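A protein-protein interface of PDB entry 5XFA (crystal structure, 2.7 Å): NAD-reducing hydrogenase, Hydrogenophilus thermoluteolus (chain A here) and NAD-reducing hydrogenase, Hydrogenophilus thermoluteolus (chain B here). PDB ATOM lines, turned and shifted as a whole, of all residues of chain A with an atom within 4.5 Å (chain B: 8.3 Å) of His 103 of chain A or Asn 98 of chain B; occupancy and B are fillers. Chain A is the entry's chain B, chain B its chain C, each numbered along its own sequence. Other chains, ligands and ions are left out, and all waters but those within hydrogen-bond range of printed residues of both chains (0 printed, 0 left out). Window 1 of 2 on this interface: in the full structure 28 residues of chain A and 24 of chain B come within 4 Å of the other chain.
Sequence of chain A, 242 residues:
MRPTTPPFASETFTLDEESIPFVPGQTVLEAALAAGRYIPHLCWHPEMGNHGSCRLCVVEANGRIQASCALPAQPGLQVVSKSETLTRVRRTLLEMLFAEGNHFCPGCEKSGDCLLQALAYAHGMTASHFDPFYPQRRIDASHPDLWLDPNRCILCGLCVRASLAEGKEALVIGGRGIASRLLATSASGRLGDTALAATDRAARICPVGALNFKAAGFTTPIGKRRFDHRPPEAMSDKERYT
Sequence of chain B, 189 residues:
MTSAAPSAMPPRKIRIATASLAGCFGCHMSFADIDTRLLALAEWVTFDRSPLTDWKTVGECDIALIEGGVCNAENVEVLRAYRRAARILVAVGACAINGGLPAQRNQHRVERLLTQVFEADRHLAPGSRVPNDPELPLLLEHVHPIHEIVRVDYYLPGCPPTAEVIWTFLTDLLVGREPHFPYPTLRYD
CZ of Phe 98 of chain A touches CE2 of Tyr 188 of chain B, 3.9 Å away. CE1 of Phe 104 of chain A touches O of Asn 98 of chain B, at 3.8 Å. O of Gly 100 of chain B touches CE1 of Phe 104 of chain A, at 3.5 Å. CB of Phe 104 of chain A touches CD1 of Leu 101 of chain B, 3.6 Å away. Ala 103 of chain B touches Phe 104 of chain A. Phe 104 of chain A touches Gln 104 of chain B (CE2 to NE2, 3.5 Å). Pro 145 of chain B touches Pro 132 of chain A (CG to CD, 3.9 Å). Tyr 134 of chain A touches Gly 99 of chain B (OH to CA, 3.7 Å). Tyr 134 of chain A touches Asn 106 of chain B (CD2 to ND2, 3.4 Å). Val 143 of chain B touches Tyr 134 of chain A.
No residue of chain B comes within 4 Å of Gly 101 of chain A. Of chain B, only Asn 98 comes within 4 Å of His 103 of chain A. Leu 116 of chain A touches none of the printed residues of chain B. Of the printed residues of chain B, Pro 132 of chain A touches Pro 145 (3.9 Å). Asn 98 of chain B touches just these residues of chain A: His 103, Phe 104 and Tyr 134. Of the printed residues of chain A, Gly 100 of chain B touches Phe 104 (3.5 Å). Pro 102 of chain B touches none of the printed residues of chain A. Printed residues of chain A within 4 Å of Asn 106 of chain B: Tyr 134 (3.4 Å). Of the printed residues of chain A, Pro 145 of chain B touches Pro 132 (3.9 Å) and Tyr 134 (3.4 Å). Printed residues of chain A within 4 Å of Tyr 188 of chain B: Phe 98 (3.9 Å) and Cys 105 (3.9 Å). The nearest residue of chain B that does not touch His 103 of chain A is Tyr 188 of chain B (6.3 Å). The nearest residue of chain A that does not touch Asn 98 of chain B is Pro 132 of chain A (4.3 Å).
Of the 27 printed residues of chain B, 10 touch a printed residue of chain A. Hydrophobic or aromatic side chains of chain B that line the printed part of chain A: Leu 101, Ala 103, Pro 145 and Tyr 188. Of the 12 printed residues of chain A, 6 touch a printed residue of chain B. Hydrophobic or aromatic side chains of chain A that line the printed part of chain B: Phe 98, Phe 104, Pro 132 and Tyr 134. Along chain A the printed residues that touch a printed residue of chain B span positions 98 to 134. Among the printed residues, 15 pairs touch across the chains.
ND2 of Asn 98 of chain B sits at hydrogen-bond distance from O of His 103 of chain A. OH of Tyr 134 of chain A is in hydrogen-bond range of O of Asn 98 of chain B, 2.7 Å away.
N of Val 143 of chain B lies within hydrogen-bond range of OD1 of Asn 106 of chain B, at 2.8 Å. The side-chain amide oxygen of Asn 98 of chain B sits close to the backbone carbonyl oxygen of Ala 94 of chain B, 3.1 Å away. The side-chain amide oxygen (OD1) of Asn 98 of chain B sits at hydrogen-bond distance from the backbone NH (N) of Gly 100 of chain B. The backbone NH (N) of Gly 100 of chain B is in hydrogen-bond range of the backbone carbonyl oxygen (O) of Ala 94 of chain B, at 3.3 Å.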
ATOM      1  N   LEU A  97     -20.607  -0.525 -17.275  1.00  0.00           N
ATOM      2  CA  LEU A  97     -19.984   0.490 -16.435  1.00  0.00           C
ATOM      3  C   LEU A  97     -20.403   1.881 -16.861  1.00  0.00           C
ATOM      4  O   LEU A  97     -20.690   2.725 -16.017  1.00  0.00           O
ATOM      5  CB  LEU A  97     -18.465   0.326 -16.464  1.00  0.00           C
ATOM      6  CG  LEU A  97     -17.991  -0.900 -15.655  1.00  0.00           C
ATOM      7  CD1 LEU A  97     -16.483  -1.105 -15.774  1.00  0.00           C
ATOM      8  CD2 LEU A  97     -18.394  -0.792 -14.189  1.00  0.00           C
ATOM      9  N   PHE A  98     -20.440   2.111 -18.175  1.00  0.00           N
ATOM     10  CA  PHE A  98     -20.933   3.362 -18.705  1.00  0.00           C
ATOM     11  C   PHE A  98     -22.413   3.553 -18.365  1.00  0.00           C
ATOM     12  O   PHE A  98     -22.809   4.613 -17.863  1.00  0.00           O
ATOM     13  CB  PHE A  98     -20.715   3.422 -20.199  1.00  0.00           C
ATOM     14  CG  PHE A  98     -19.375   3.973 -20.594  1.00  0.00           C
ATOM     15  CD1 PHE A  98     -18.271   3.146 -20.720  1.00  0.00           C
ATOM     16  CD2 PHE A  98     -19.211   5.310 -20.859  1.00  0.00           C
ATOM     17  CE1 PHE A  98     -17.024   3.644 -21.084  1.00  0.00           C
ATOM     18  CE2 PHE A  98     -17.972   5.805 -21.240  1.00  0.00           C
ATOM     19  CZ  PHE A  98     -16.879   4.972 -21.351  1.00  0.00           C
ATOM     20  N   GLY A 101     -23.057   4.479 -14.430  1.00  0.00           N
ATOM     21  CA  GLY A 101     -22.746   5.817 -13.914  1.00  0.00           C
ATOM     22  C   GLY A 101     -23.085   6.937 -14.908  1.00  0.00           C
ATOM     23  O   GLY A 101     -23.626   6.706 -16.006  1.00  0.00           O
ATOM     24  N   ASN A 102     -22.765   8.169 -14.517  1.00  0.00           N
ATOM     25  CA  ASN A 102     -22.974   9.320 -15.366  1.00  0.00           C
ATOM     26  C   ASN A 102     -21.637   9.644 -16.016  1.00  0.00           C
ATOM     27  O   ASN A 102     -20.864  10.479 -15.525  1.00  0.00           O
ATOM     28  CB  ASN A 102     -23.493  10.510 -14.560  1.00  0.00           C
ATOM     29  CG  ASN A 102     -24.796  10.209 -13.841  1.00  0.00           C
ATOM     30  OD1 ASN A 102     -25.673   9.505 -14.359  1.00  0.00           O
ATOM     31  ND2 ASN A 102     -24.927  10.727 -12.620  1.00  0.00           N
ATOM     32  N   HIS A 103     -21.359   8.935 -17.104  1.00  0.00           N
ATOM     33  CA  HIS A 103     -20.197   9.206 -17.932  1.00  0.00           C
ATOM     34  C   HIS A 103     -20.586  10.022 -19.167  1.00  0.00           C
ATOM     35  O   HIS A 103     -20.605   9.566 -20.327  1.00  0.00           O
ATOM     36  CB  HIS A 103     -19.490   7.917 -18.285  1.00  0.00           C
ATOM     37  CG  HIS A 103     -19.164   7.114 -17.089  1.00  0.00           C
ATOM     38  ND1 HIS A 103     -18.009   7.292 -16.373  1.00  0.00           N
ATOM     39  CD2 HIS A 103     -19.899   6.212 -16.412  1.00  0.00           C
ATOM     40  CE1 HIS A 103     -18.019   6.490 -15.336  1.00  0.00           C
ATOM     41  NE2 HIS A 103     -19.151   5.815 -15.342  1.00  0.00           N
ATOM     42  N   PHE A 104     -20.877  11.263 -18.820  1.00  0.00           N
ATOM     43  CA  PHE A 104     -20.854  12.393 -19.662  1.00  0.00           C
ATOM     44  C   PHE A 104     -19.411  12.864 -19.824  1.00  0.00           C
ATOM     45  O   PHE A 104     -19.050  13.927 -19.325  1.00  0.00           O
ATOM     46  CB  PHE A 104     -21.663  13.482 -18.944  1.00  0.00           C
ATOM     47  CG  PHE A 104     -23.029  13.019 -18.523  1.00  0.00           C
ATOM     48  CD1 PHE A 104     -23.784  12.187 -19.345  1.00  0.00           C
ATOM     49  CD2 PHE A 104     -23.561  13.395 -17.323  1.00  0.00           C
ATOM     50  CE1 PHE A 104     -25.043  11.737 -18.981  1.00  0.00           C
ATOM     51  CE2 PHE A 104     -24.823  12.952 -16.953  1.00  0.00           C
ATOM     52  CZ  PHE A 104     -25.563  12.115 -17.778  1.00  0.00           C
ATOM     53  N   CYS A 105     -18.585  12.120 -20.551  1.00  0.00           N
ATOM     54  CA  CYS A 105     -17.221  12.579 -20.840  1.00  0.00           C
ATOM     55  C   CYS A 105     -17.105  14.055 -21.316  1.00  0.00           C
ATOM     56  O   CYS A 105     -16.105  14.691 -21.012  1.00  0.00           O
ATOM     57  CB  CYS A 105     -16.562  11.686 -21.895  1.00  0.00           C
ATOM     58  SG  CYS A 105     -16.697   9.915 -21.568  1.00  0.00           S
ATOM     59  N   LEU A 116     -11.020   3.927 -18.448  1.00  0.00           N
ATOM     60  CA  LEU A 116     -12.304   3.378 -18.827  1.00  0.00           C
ATOM     61  C   LEU A 116     -12.641   3.840 -20.230  1.00  0.00           C
ATOM     62  O   LEU A 116     -12.974   3.030 -21.098  1.00  0.00           O
ATOM     63  CB  LEU A 116     -13.385   3.824 -17.848  1.00  0.00           C
ATOM     64  CG  LEU A 116     -14.841   3.633 -18.283  1.00  0.00           C
ATOM     65  CD1 LEU A 116     -15.116   2.192 -18.624  1.00  0.00           C
ATOM     66  CD2 LEU A 116     -15.805   4.107 -17.214  1.00  0.00           C
ATOM     67  N   PRO A 132     -29.599   3.910 -19.135  1.00  0.00           N
ATOM     68  CA  PRO A 132     -28.840   4.523 -18.050  1.00  0.00           C
ATOM     69  C   PRO A 132     -29.482   4.344 -16.669  1.00  0.00           C
ATOM     70  O   PRO A 132     -30.693   4.264 -16.549  1.00  0.00           O
ATOM     71  CB  PRO A 132     -28.839   6.019 -18.425  1.00  0.00           C
ATOM     72  CG  PRO A 132     -29.088   6.076 -19.884  1.00  0.00           C
ATOM     73  CD  PRO A 132     -29.912   4.875 -20.215  1.00  0.00           C
ATOM     74  N   TYR A 134     -28.753   6.603 -14.206  1.00  0.00           N
ATOM     75  CA  TYR A 134     -28.776   7.975 -13.679  1.00  0.00           C
ATOM     76  C   TYR A 134     -28.749   8.016 -12.158  1.00  0.00           C
ATOM     77  O   TYR A 134     -29.650   8.562 -11.541  1.00  0.00           O
ATOM     78  CB  TYR A 134     -30.001   8.727 -14.203  1.00  0.00           C
ATOM     79  CG  TYR A 134     -29.955   8.993 -15.677  1.00  0.00           C
ATOM     80  CD1 TYR A 134     -28.837   9.593 -16.251  1.00  0.00           C
ATOM     81  CD2 TYR A 134     -31.032   8.683 -16.507  1.00  0.00           C
ATOM     82  CE1 TYR A 134     -28.770   9.864 -17.602  1.00  0.00           C
ATOM     83  CE2 TYR A 134     -30.971   8.946 -17.874  1.00  0.00           C
ATOM     84  CZ  TYR A 134     -29.824   9.542 -18.404  1.00  0.00           C
ATOM     85  OH  TYR A 134     -29.702   9.815 -19.737  1.00  0.00           O
ATOM     86  N   ASN A 151     -20.466   9.493  -9.084  1.00  0.00           N
ATOM     87  CA  ASN A 151     -21.283   8.982 -10.190  1.00  0.00           C
ATOM     88  C   ASN A 151     -20.458   8.538 -11.391  1.00  0.00           C
ATOM     89  O   ASN A 151     -20.995   7.980 -12.349  1.00  0.00           O
ATOM     90  CB  ASN A 151     -22.321  10.028 -10.603  1.00  0.00           C
ATOM     91  CG  ASN A 151     -23.362  10.259  -9.524  1.00  0.00           C
ATOM     92  OD1 ASN A 151     -24.080   9.324  -9.128  1.00  0.00           O
ATOM     93  ND2 ASN A 151     -23.409  11.466  -8.994  1.00  0.00           N
ATOM     94  N   ARG A 152     -19.156   8.796 -11.308  1.00  0.00           N
ATOM     95  CA  ARG A 152     -18.153   8.316 -12.240  1.00  0.00           C
ATOM     96  C   ARG A 152     -17.357   7.092 -11.714  1.00  0.00           C
ATOM     97  O   ARG A 152     -16.657   6.431 -12.478  1.00  0.00           O
ATOM     98  CB  ARG A 152     -17.180   9.466 -12.530  1.00  0.00           C
ATOM     99  CG  ARG A 152     -17.813  10.595 -13.340  1.00  0.00           C
ATOM    100  CD  ARG A 152     -16.929  11.812 -13.369  1.00  0.00           C
ATOM    101  NE  ARG A 152     -17.516  12.905 -14.146  1.00  0.00           N
ATOM    102  CZ  ARG A 152     -17.042  14.149 -14.133  1.00  0.00           C
ATOM    103  NH1 ARG A 152     -15.971  14.458 -13.399  1.00  0.00           N
ATOM    104  NH2 ARG A 152     -17.615  15.093 -14.864  1.00  0.00           N
ATOM    105  N   GLY B  68     -29.480  15.186 -29.996  1.00  0.00           N
ATOM    106  CA  GLY B  68     -30.153  15.659 -28.796  1.00  0.00           C
ATOM    107  C   GLY B  68     -30.897  14.587 -28.045  1.00  0.00           C
ATOM    108  O   GLY B  68     -31.322  13.602 -28.639  1.00  0.00           O
ATOM    109  N   GLY B  69     -31.047  14.783 -26.728  1.00  0.00           N
ATOM    110  CA  GLY B  69     -31.802  13.850 -25.872  1.00  0.00           C
ATOM    111  C   GLY B  69     -33.294  14.091 -26.006  1.00  0.00           C
ATOM    112  O   GLY B  69     -33.708  14.856 -26.867  1.00  0.00           O
ATOM    113  N   VAL B  70     -34.116  13.417 -25.203  1.00  0.00           N
ATOM    114  CA  VAL B  70     -35.544  13.785 -25.118  1.00  0.00           C
ATOM    115  C   VAL B  70     -35.756  14.389 -23.752  1.00  0.00           C
ATOM    116  O   VAL B  70     -35.438  13.772 -22.723  1.00  0.00           O
ATOM    117  CB  VAL B  70     -36.540  12.641 -25.417  1.00  0.00           C
ATOM    118  CG1 VAL B  70     -36.230  12.039 -26.773  1.00  0.00           C
ATOM    119  CG2 VAL B  70     -36.513  11.567 -24.350  1.00  0.00           C
ATOM    120  N   ALA B  91     -28.758   7.826 -33.950  1.00  0.00           N
ATOM    121  CA  ALA B  91     -28.524   8.650 -32.778  1.00  0.00           C
ATOM    122  C   ALA B  91     -27.120   9.255 -32.865  1.00  0.00           C
ATOM    123  O   ALA B  91     -26.096   8.585 -32.712  1.00  0.00           O
ATOM    124  CB  ALA B  91     -28.676   7.844 -31.504  1.00  0.00           C
ATOM    125  N   VAL B  92     -27.119  10.552 -33.092  1.00  0.00           N
ATOM    126  CA  VAL B  92     -25.941  11.342 -33.345  1.00  0.00           C
ATOM    127  C   VAL B  92     -25.608  12.120 -32.081  1.00  0.00           C
ATOM    128  O   VAL B  92     -26.493  12.706 -31.438  1.00  0.00           O
ATOM    129  CB  VAL B  92     -26.249  12.327 -34.500  1.00  0.00           C
ATOM    130  CG1 VAL B  92     -25.089  13.251 -34.757  1.00  0.00           C
ATOM    131  CG2 VAL B  92     -26.564  11.549 -35.745  1.00  0.00           C
ATOM    132  N   GLY B  93     -24.344  12.148 -31.725  1.00  0.00           N
ATOM    133  CA  GLY B  93     -23.905  12.902 -30.547  1.00  0.00           C
ATOM    134  C   GLY B  93     -24.170  12.300 -29.172  1.00  0.00           C
ATOM    135  O   GLY B  93     -25.092  11.515 -28.981  1.00  0.00           O
ATOM    136  N   ALA B  94     -23.374  12.728 -28.207  1.00  0.00           N
ATOM    137  CA  ALA B  94     -23.541  12.338 -26.802  1.00  0.00           C
ATOM    138  C   ALA B  94     -24.941  12.506 -26.235  1.00  0.00           C
ATOM    139  O   ALA B  94     -25.419  11.676 -25.472  1.00  0.00           O
ATOM    140  CB  ALA B  94     -22.596  13.149 -25.948  1.00  0.00           C
ATOM    141  N   CYS B  95     -25.578  13.613 -26.582  1.00  0.00           N
ATOM    142  CA  CYS B  95     -26.927  13.901 -26.108  1.00  0.00           C
ATOM    143  C   CYS B  95     -27.876  12.746 -26.425  1.00  0.00           C
ATOM    144  O   CYS B  95     -28.581  12.263 -25.547  1.00  0.00           O
ATOM    145  CB  CYS B  95     -27.474  15.172 -26.792  1.00  0.00           C
ATOM    146  SG  CYS B  95     -26.896  16.732 -26.122  1.00  0.00           S
ATOM    147  N   ALA B  96     -27.910  12.347 -27.697  1.00  0.00           N
ATOM    148  CA  ALA B  96     -28.885  11.365 -28.163  1.00  0.00           C
ATOM    149  C   ALA B  96     -28.492   9.980 -27.704  1.00  0.00           C
ATOM    150  O   ALA B  96     -29.345   9.106 -27.485  1.00  0.00           O
ATOM    151  CB  ALA B  96     -29.016  11.424 -29.686  1.00  0.00           C
ATOM    152  N   ILE B  97     -27.194   9.790 -27.536  1.00  0.00           N
ATOM    153  CA  ILE B  97     -26.649   8.490 -27.096  1.00  0.00           C
ATOM    154  C   ILE B  97     -26.949   8.113 -25.637  1.00  0.00           C
ATOM    155  O   ILE B  97     -27.544   7.071 -25.397  1.00  0.00           O
ATOM    156  CB  ILE B  97     -25.127   8.411 -27.376  1.00  0.00           C
ATOM    157  CG1 ILE B  97     -24.914   8.150 -28.865  1.00  0.00           C
ATOM    158  CG2 ILE B  97     -24.454   7.341 -26.533  1.00  0.00           C
ATOM    159  CD1 ILE B  97     -23.543   8.532 -29.365  1.00  0.00           C
ATOM    160  N   ASN B  98     -26.529   8.935 -24.687  1.00  0.00           N
ATOM    161  CA  ASN B  98     -26.796   8.668 -23.248  1.00  0.00           C
ATOM    162  C   ASN B  98     -27.445   9.825 -22.440  1.00  0.00           C
ATOM    163  O   ASN B  98     -27.409   9.825 -21.191  1.00  0.00           O
ATOM    164  CB  ASN B  98     -25.515   8.219 -22.545  1.00  0.00           C
ATOM    165  CG  ASN B  98     -24.527   9.366 -22.300  1.00  0.00           C
ATOM    166  OD1 ASN B  98     -24.765  10.541 -22.626  1.00  0.00           O
ATOM    167  ND2 ASN B  98     -23.406   9.015 -21.693  1.00  0.00           N
ATOM    168  N   GLY B  99     -27.994  10.808 -23.166  1.00  0.00           N
ATOM    169  CA  GLY B  99     -28.646  11.959 -22.561  1.00  0.00           C
ATOM    170  C   GLY B  99     -27.780  13.204 -22.481  1.00  0.00           C
ATOM    171  O   GLY B  99     -28.301  14.301 -22.271  1.00  0.00           O
ATOM    172  N   GLY B 100     -26.468  13.033 -22.629  1.00  0.00           N
ATOM    173  CA  GLY B 100     -25.509  14.144 -22.614  1.00  0.00           C
ATOM    174  C   GLY B 100     -25.468  14.983 -21.352  1.00  0.00           C
ATOM    175  O   GLY B 100     -26.192  14.743 -20.395  1.00  0.00           O
ATOM    176  N   LEU B 101     -24.634  16.011 -21.387  1.00  0.00           N
ATOM    177  CA  LEU B 101     -24.613  17.045 -20.336  1.00  0.00           C
ATOM    178  C   LEU B 101     -25.984  17.635 -19.886  1.00  0.00           C
ATOM    179  O   LEU B 101     -26.142  18.035 -18.739  1.00  0.00           O
ATOM    180  CB  LEU B 101     -23.670  18.189 -20.755  1.00  0.00           C
ATOM    181  CG  LEU B 101     -22.274  18.261 -20.141  1.00  0.00           C
ATOM    182  CD1 LEU B 101     -21.626  16.904 -19.938  1.00  0.00           C
ATOM    183  CD2 LEU B 101     -21.380  19.145 -20.982  1.00  0.00           C
ATOM    184  N   PRO B 102     -26.959  17.742 -20.790  1.00  0.00           N
ATOM    185  CA  PRO B 102     -28.271  18.160 -20.290  1.00  0.00           C
ATOM    186  C   PRO B 102     -28.808  17.217 -19.260  1.00  0.00           C
ATOM    187  O   PRO B 102     -29.488  17.638 -18.329  1.00  0.00           O
ATOM    188  CB  PRO B 102     -29.151  18.110 -21.531  1.00  0.00           C
ATOM    189  CG  PRO B 102     -28.212  18.443 -22.645  1.00  0.00           C
ATOM    190  CD  PRO B 102     -26.864  17.880 -22.260  1.00  0.00           C
ATOM    191  N   ALA B 103     -28.475  15.942 -19.400  1.00  0.00           N
ATOM    192  CA  ALA B 103     -28.929  14.935 -18.445  1.00  0.00           C
ATOM    193  C   ALA B 103     -28.354  15.045 -17.029  1.00  0.00           C
ATOM    194  O   ALA B 103     -28.757  14.301 -16.147  1.00  0.00           O
ATOM    195  CB  ALA B 103     -28.692  13.560 -18.992  1.00  0.00           C
ATOM    196  N   GLN B 104     -27.456  15.992 -16.807  1.00  0.00           N
ATOM    197  CA  GLN B 104     -27.039  16.350 -15.458  1.00  0.00           C
ATOM    198  C   GLN B 104     -28.213  16.909 -14.658  1.00  0.00           C
ATOM    199  O   GLN B 104     -28.136  16.984 -13.441  1.00  0.00           O
ATOM    200  CB  GLN B 104     -25.903  17.393 -15.498  1.00  0.00           C
ATOM    201  CG  GLN B 104     -24.615  16.907 -16.138  1.00  0.00           C
ATOM    202  CD  GLN B 104     -23.682  16.242 -15.135  1.00  0.00           C
ATOM    203  OE1 GLN B 104     -22.509  16.606 -15.040  1.00  0.00           O
ATOM    204  NE2 GLN B 104     -24.199  15.279 -14.367  1.00  0.00           N
ATOM    205  N   ASN B 106     -31.025  15.468 -14.285  1.00  0.00           N
ATOM    206  CA  ASN B 106     -31.589  14.305 -13.574  1.00  0.00           C
ATOM    207  C   ASN B 106     -31.088  14.132 -12.118  1.00  0.00           C
ATOM    208  O   ASN B 106     -31.659  13.363 -11.335  1.00  0.00           O
ATOM    209  CB  ASN B 106     -31.296  13.046 -14.366  1.00  0.00           C
ATOM    210  CG  ASN B 106     -31.901  13.081 -15.743  1.00  0.00           C
ATOM    211  OD1 ASN B 106     -32.432  14.100 -16.164  1.00  0.00           O
ATOM    212  ND2 ASN B 106     -31.850  11.964 -16.443  1.00  0.00           N
ATOM    213  N   VAL B 143     -34.313  13.667 -18.239  1.00  0.00           N
ATOM    214  CA  VAL B 143     -33.838  13.589 -19.628  1.00  0.00           C
ATOM    215  C   VAL B 143     -33.452  12.143 -19.932  1.00  0.00           C
ATOM    216  O   VAL B 143     -32.858  11.479 -19.076  1.00  0.00           O
ATOM    217  CB  VAL B 143     -32.593  14.456 -19.835  1.00  0.00           C
ATOM    218  CG1 VAL B 143     -32.070  14.306 -21.249  1.00  0.00           C
ATOM    219  CG2 VAL B 143     -32.910  15.910 -19.543  1.00  0.00           C
ATOM    220  N   HIS B 144     -33.783  11.672 -21.138  1.00  0.00           N
ATOM    221  CA  HIS B 144     -33.512  10.290 -21.561  1.00  0.00           C
ATOM    222  C   HIS B 144     -32.822  10.244 -22.935  1.00  0.00           C
ATOM    223  O   HIS B 144     -33.119  11.059 -23.797  1.00  0.00           O
ATOM    224  CB  HIS B 144     -34.825   9.495 -21.685  1.00  0.00           C
ATOM    225  CG  HIS B 144     -35.743   9.601 -20.506  1.00  0.00           C
ATOM    226  ND1 HIS B 144     -35.780   8.665 -19.494  1.00  0.00           N
ATOM    227  CD2 HIS B 144     -36.701  10.510 -20.211  1.00  0.00           C
ATOM    228  CE1 HIS B 144     -36.692   9.016 -18.604  1.00  0.00           C
ATOM    229  NE2 HIS B 144     -37.265  10.131 -19.018  1.00  0.00           N
ATOM    230  N   PRO B 145     -31.956   9.245 -23.174  1.00  0.00           N
ATOM    231  CA  PRO B 145     -31.441   9.062 -24.527  1.00  0.00           C
ATOM    232  C   PRO B 145     -32.549   8.718 -25.495  1.00  0.00           C
ATOM    233  O   PRO B 145     -33.641   8.360 -25.045  1.00  0.00           O
ATOM    234  CB  PRO B 145     -30.480   7.865 -24.380  1.00  0.00           C
ATOM    235  CG  PRO B 145     -30.912   7.176 -23.148  1.00  0.00           C
ATOM    236  CD  PRO B 145     -31.352   8.278 -22.239  1.00  0.00           C
ATOM    237  N   ILE B 146     -32.300   8.773 -26.803  1.00  0.00           N
ATOM    238  CA  ILE B 146     -33.387   8.418 -27.717  1.00  0.00           C
ATOM    239  C   ILE B 146     -33.741   6.925 -27.655  1.00  0.00           C
ATOM    240  O   ILE B 146     -34.911   6.577 -27.796  1.00  0.00           O
ATOM    241  CB  ILE B 146     -33.151   8.853 -29.180  1.00  0.00           C
ATOM    242  CG1 ILE B 146     -32.152   7.944 -29.865  1.00  0.00           C
ATOM    243  CG2 ILE B 146     -32.693  10.308 -29.270  1.00  0.00           C
ATOM    244  CD1 ILE B 146     -31.988   8.297 -31.317  1.00  0.00           C
ATOM    245  N   HIS B 147     -32.756   6.055 -27.388  1.00  0.00           N
ATOM    246  CA  HIS B 147     -32.995   4.594 -27.389  1.00  0.00           C
ATOM    247  C   HIS B 147     -33.963   4.100 -26.308  1.00  0.00           C
ATOM    248  O   HIS B 147     -34.481   2.988 -26.380  1.00  0.00           O
ATOM    249  CB  HIS B 147     -31.684   3.770 -27.430  1.00  0.00           C
ATOM    250  CG  HIS B 147     -30.922   3.709 -26.149  1.00  0.00           C
ATOM    251  ND1 HIS B 147     -29.544   3.753 -26.115  1.00  0.00           N
ATOM    252  CD2 HIS B 147     -31.323   3.534 -24.867  1.00  0.00           C
ATOM    253  CE1 HIS B 147     -29.130   3.637 -24.866  1.00  0.00           C
ATOM    254  NE2 HIS B 147     -30.189   3.506 -24.088  1.00  0.00           N
ATOM    255  N   GLU B 148     -34.227   4.945 -25.324  1.00  0.00           N
ATOM    256  CA  GLU B 148     -35.188   4.627 -24.281  1.00  0.00           C
ATOM    257  C   GLU B 148     -36.624   4.843 -24.763  1.00  0.00           C
ATOM    258  O   GLU B 148     -37.566   4.372 -24.143  1.00  0.00           O
ATOM    259  CB  GLU B 148     -34.892   5.489 -23.057  1.00  0.00           C
ATOM    260  CG  GLU B 148     -35.092   4.769 -21.739  1.00  0.00           C
ATOM    261  CD  GLU B 148     -34.392   5.485 -20.606  1.00  0.00           C
ATOM    262  OE1 GLU B 148     -33.684   6.460 -20.894  1.00  0.00           O
ATOM    263  OE2 GLU B 148     -34.546   5.083 -19.435  1.00  0.00           O
ATOM    264  N   TYR B 155     -25.245   4.503 -33.784  1.00  0.00           N
ATOM    265  CA  TYR B 155     -24.858   5.603 -32.914  1.00  0.00           C
ATOM    266  C   TYR B 155     -23.591   6.260 -33.470  1.00  0.00           C
ATOM    267  O   TYR B 155     -22.662   5.570 -33.884  1.00  0.00           O
ATOM    268  CB  TYR B 155     -24.574   5.082 -31.497  1.00  0.00           C
ATOM    269  CG  TYR B 155     -25.699   4.303 -30.837  1.00  0.00           C
ATOM    270  CD1 TYR B 155     -25.794   2.926 -30.955  1.00  0.00           C
ATOM    271  CD2 TYR B 155     -26.675   4.955 -30.105  1.00  0.00           C
ATOM    272  CE1 TYR B 155     -26.823   2.218 -30.350  1.00  0.00           C
ATOM    273  CE2 TYR B 155     -27.702   4.261 -29.496  1.00  0.00           C
ATOM    274  CZ  TYR B 155     -27.771   2.896 -29.622  1.00  0.00           C
ATOM    275  OH  TYR B 155     -28.795   2.236 -29.000  1.00  0.00           O
ATOM    276  N   GLY B 158     -19.597  11.306 -29.817  1.00  0.00           N
ATOM    277  CA  GLY B 158     -18.905  12.597 -29.833  1.00  0.00           C
ATOM    278  C   GLY B 158     -19.816  13.707 -29.354  1.00  0.00           C
ATOM    279  O   GLY B 158     -21.036  13.553 -29.298  1.00  0.00           O
ATOM    280  N   TYR B 188     -15.859  10.602 -27.459  1.00  0.00           N
ATOM    281  CA  TYR B 188     -17.077  10.807 -26.716  1.00  0.00           C
ATOM    282  C   TYR B 188     -17.110  12.227 -26.179  1.00  0.00           C
ATOM    283  O   TYR B 188     -17.995  12.581 -25.419  1.00  0.00           O
ATOM    284  CB  TYR B 188     -17.123   9.847 -25.516  1.00  0.00           C
ATOM    285  CG  TYR B 188     -16.960   8.380 -25.805  1.00  0.00           C
ATOM    286  CD1 TYR B 188     -17.214   7.843 -27.060  1.00  0.00           C
ATOM    287  CD2 TYR B 188     -16.601   7.505 -24.781  1.00  0.00           C
ATOM    288  CE1 TYR B 188     -17.074   6.486 -27.288  1.00  0.00           C
ATOM    289  CE2 TYR B 188     -16.458   6.155 -24.998  1.00  0.00           C
ATOM    290  CZ  TYR B 188     -16.685   5.650 -26.248  1.00  0.00           C
ATOM    291  OH  TYR B 188     -16.530   4.305 -26.429  1.00  0.00           O
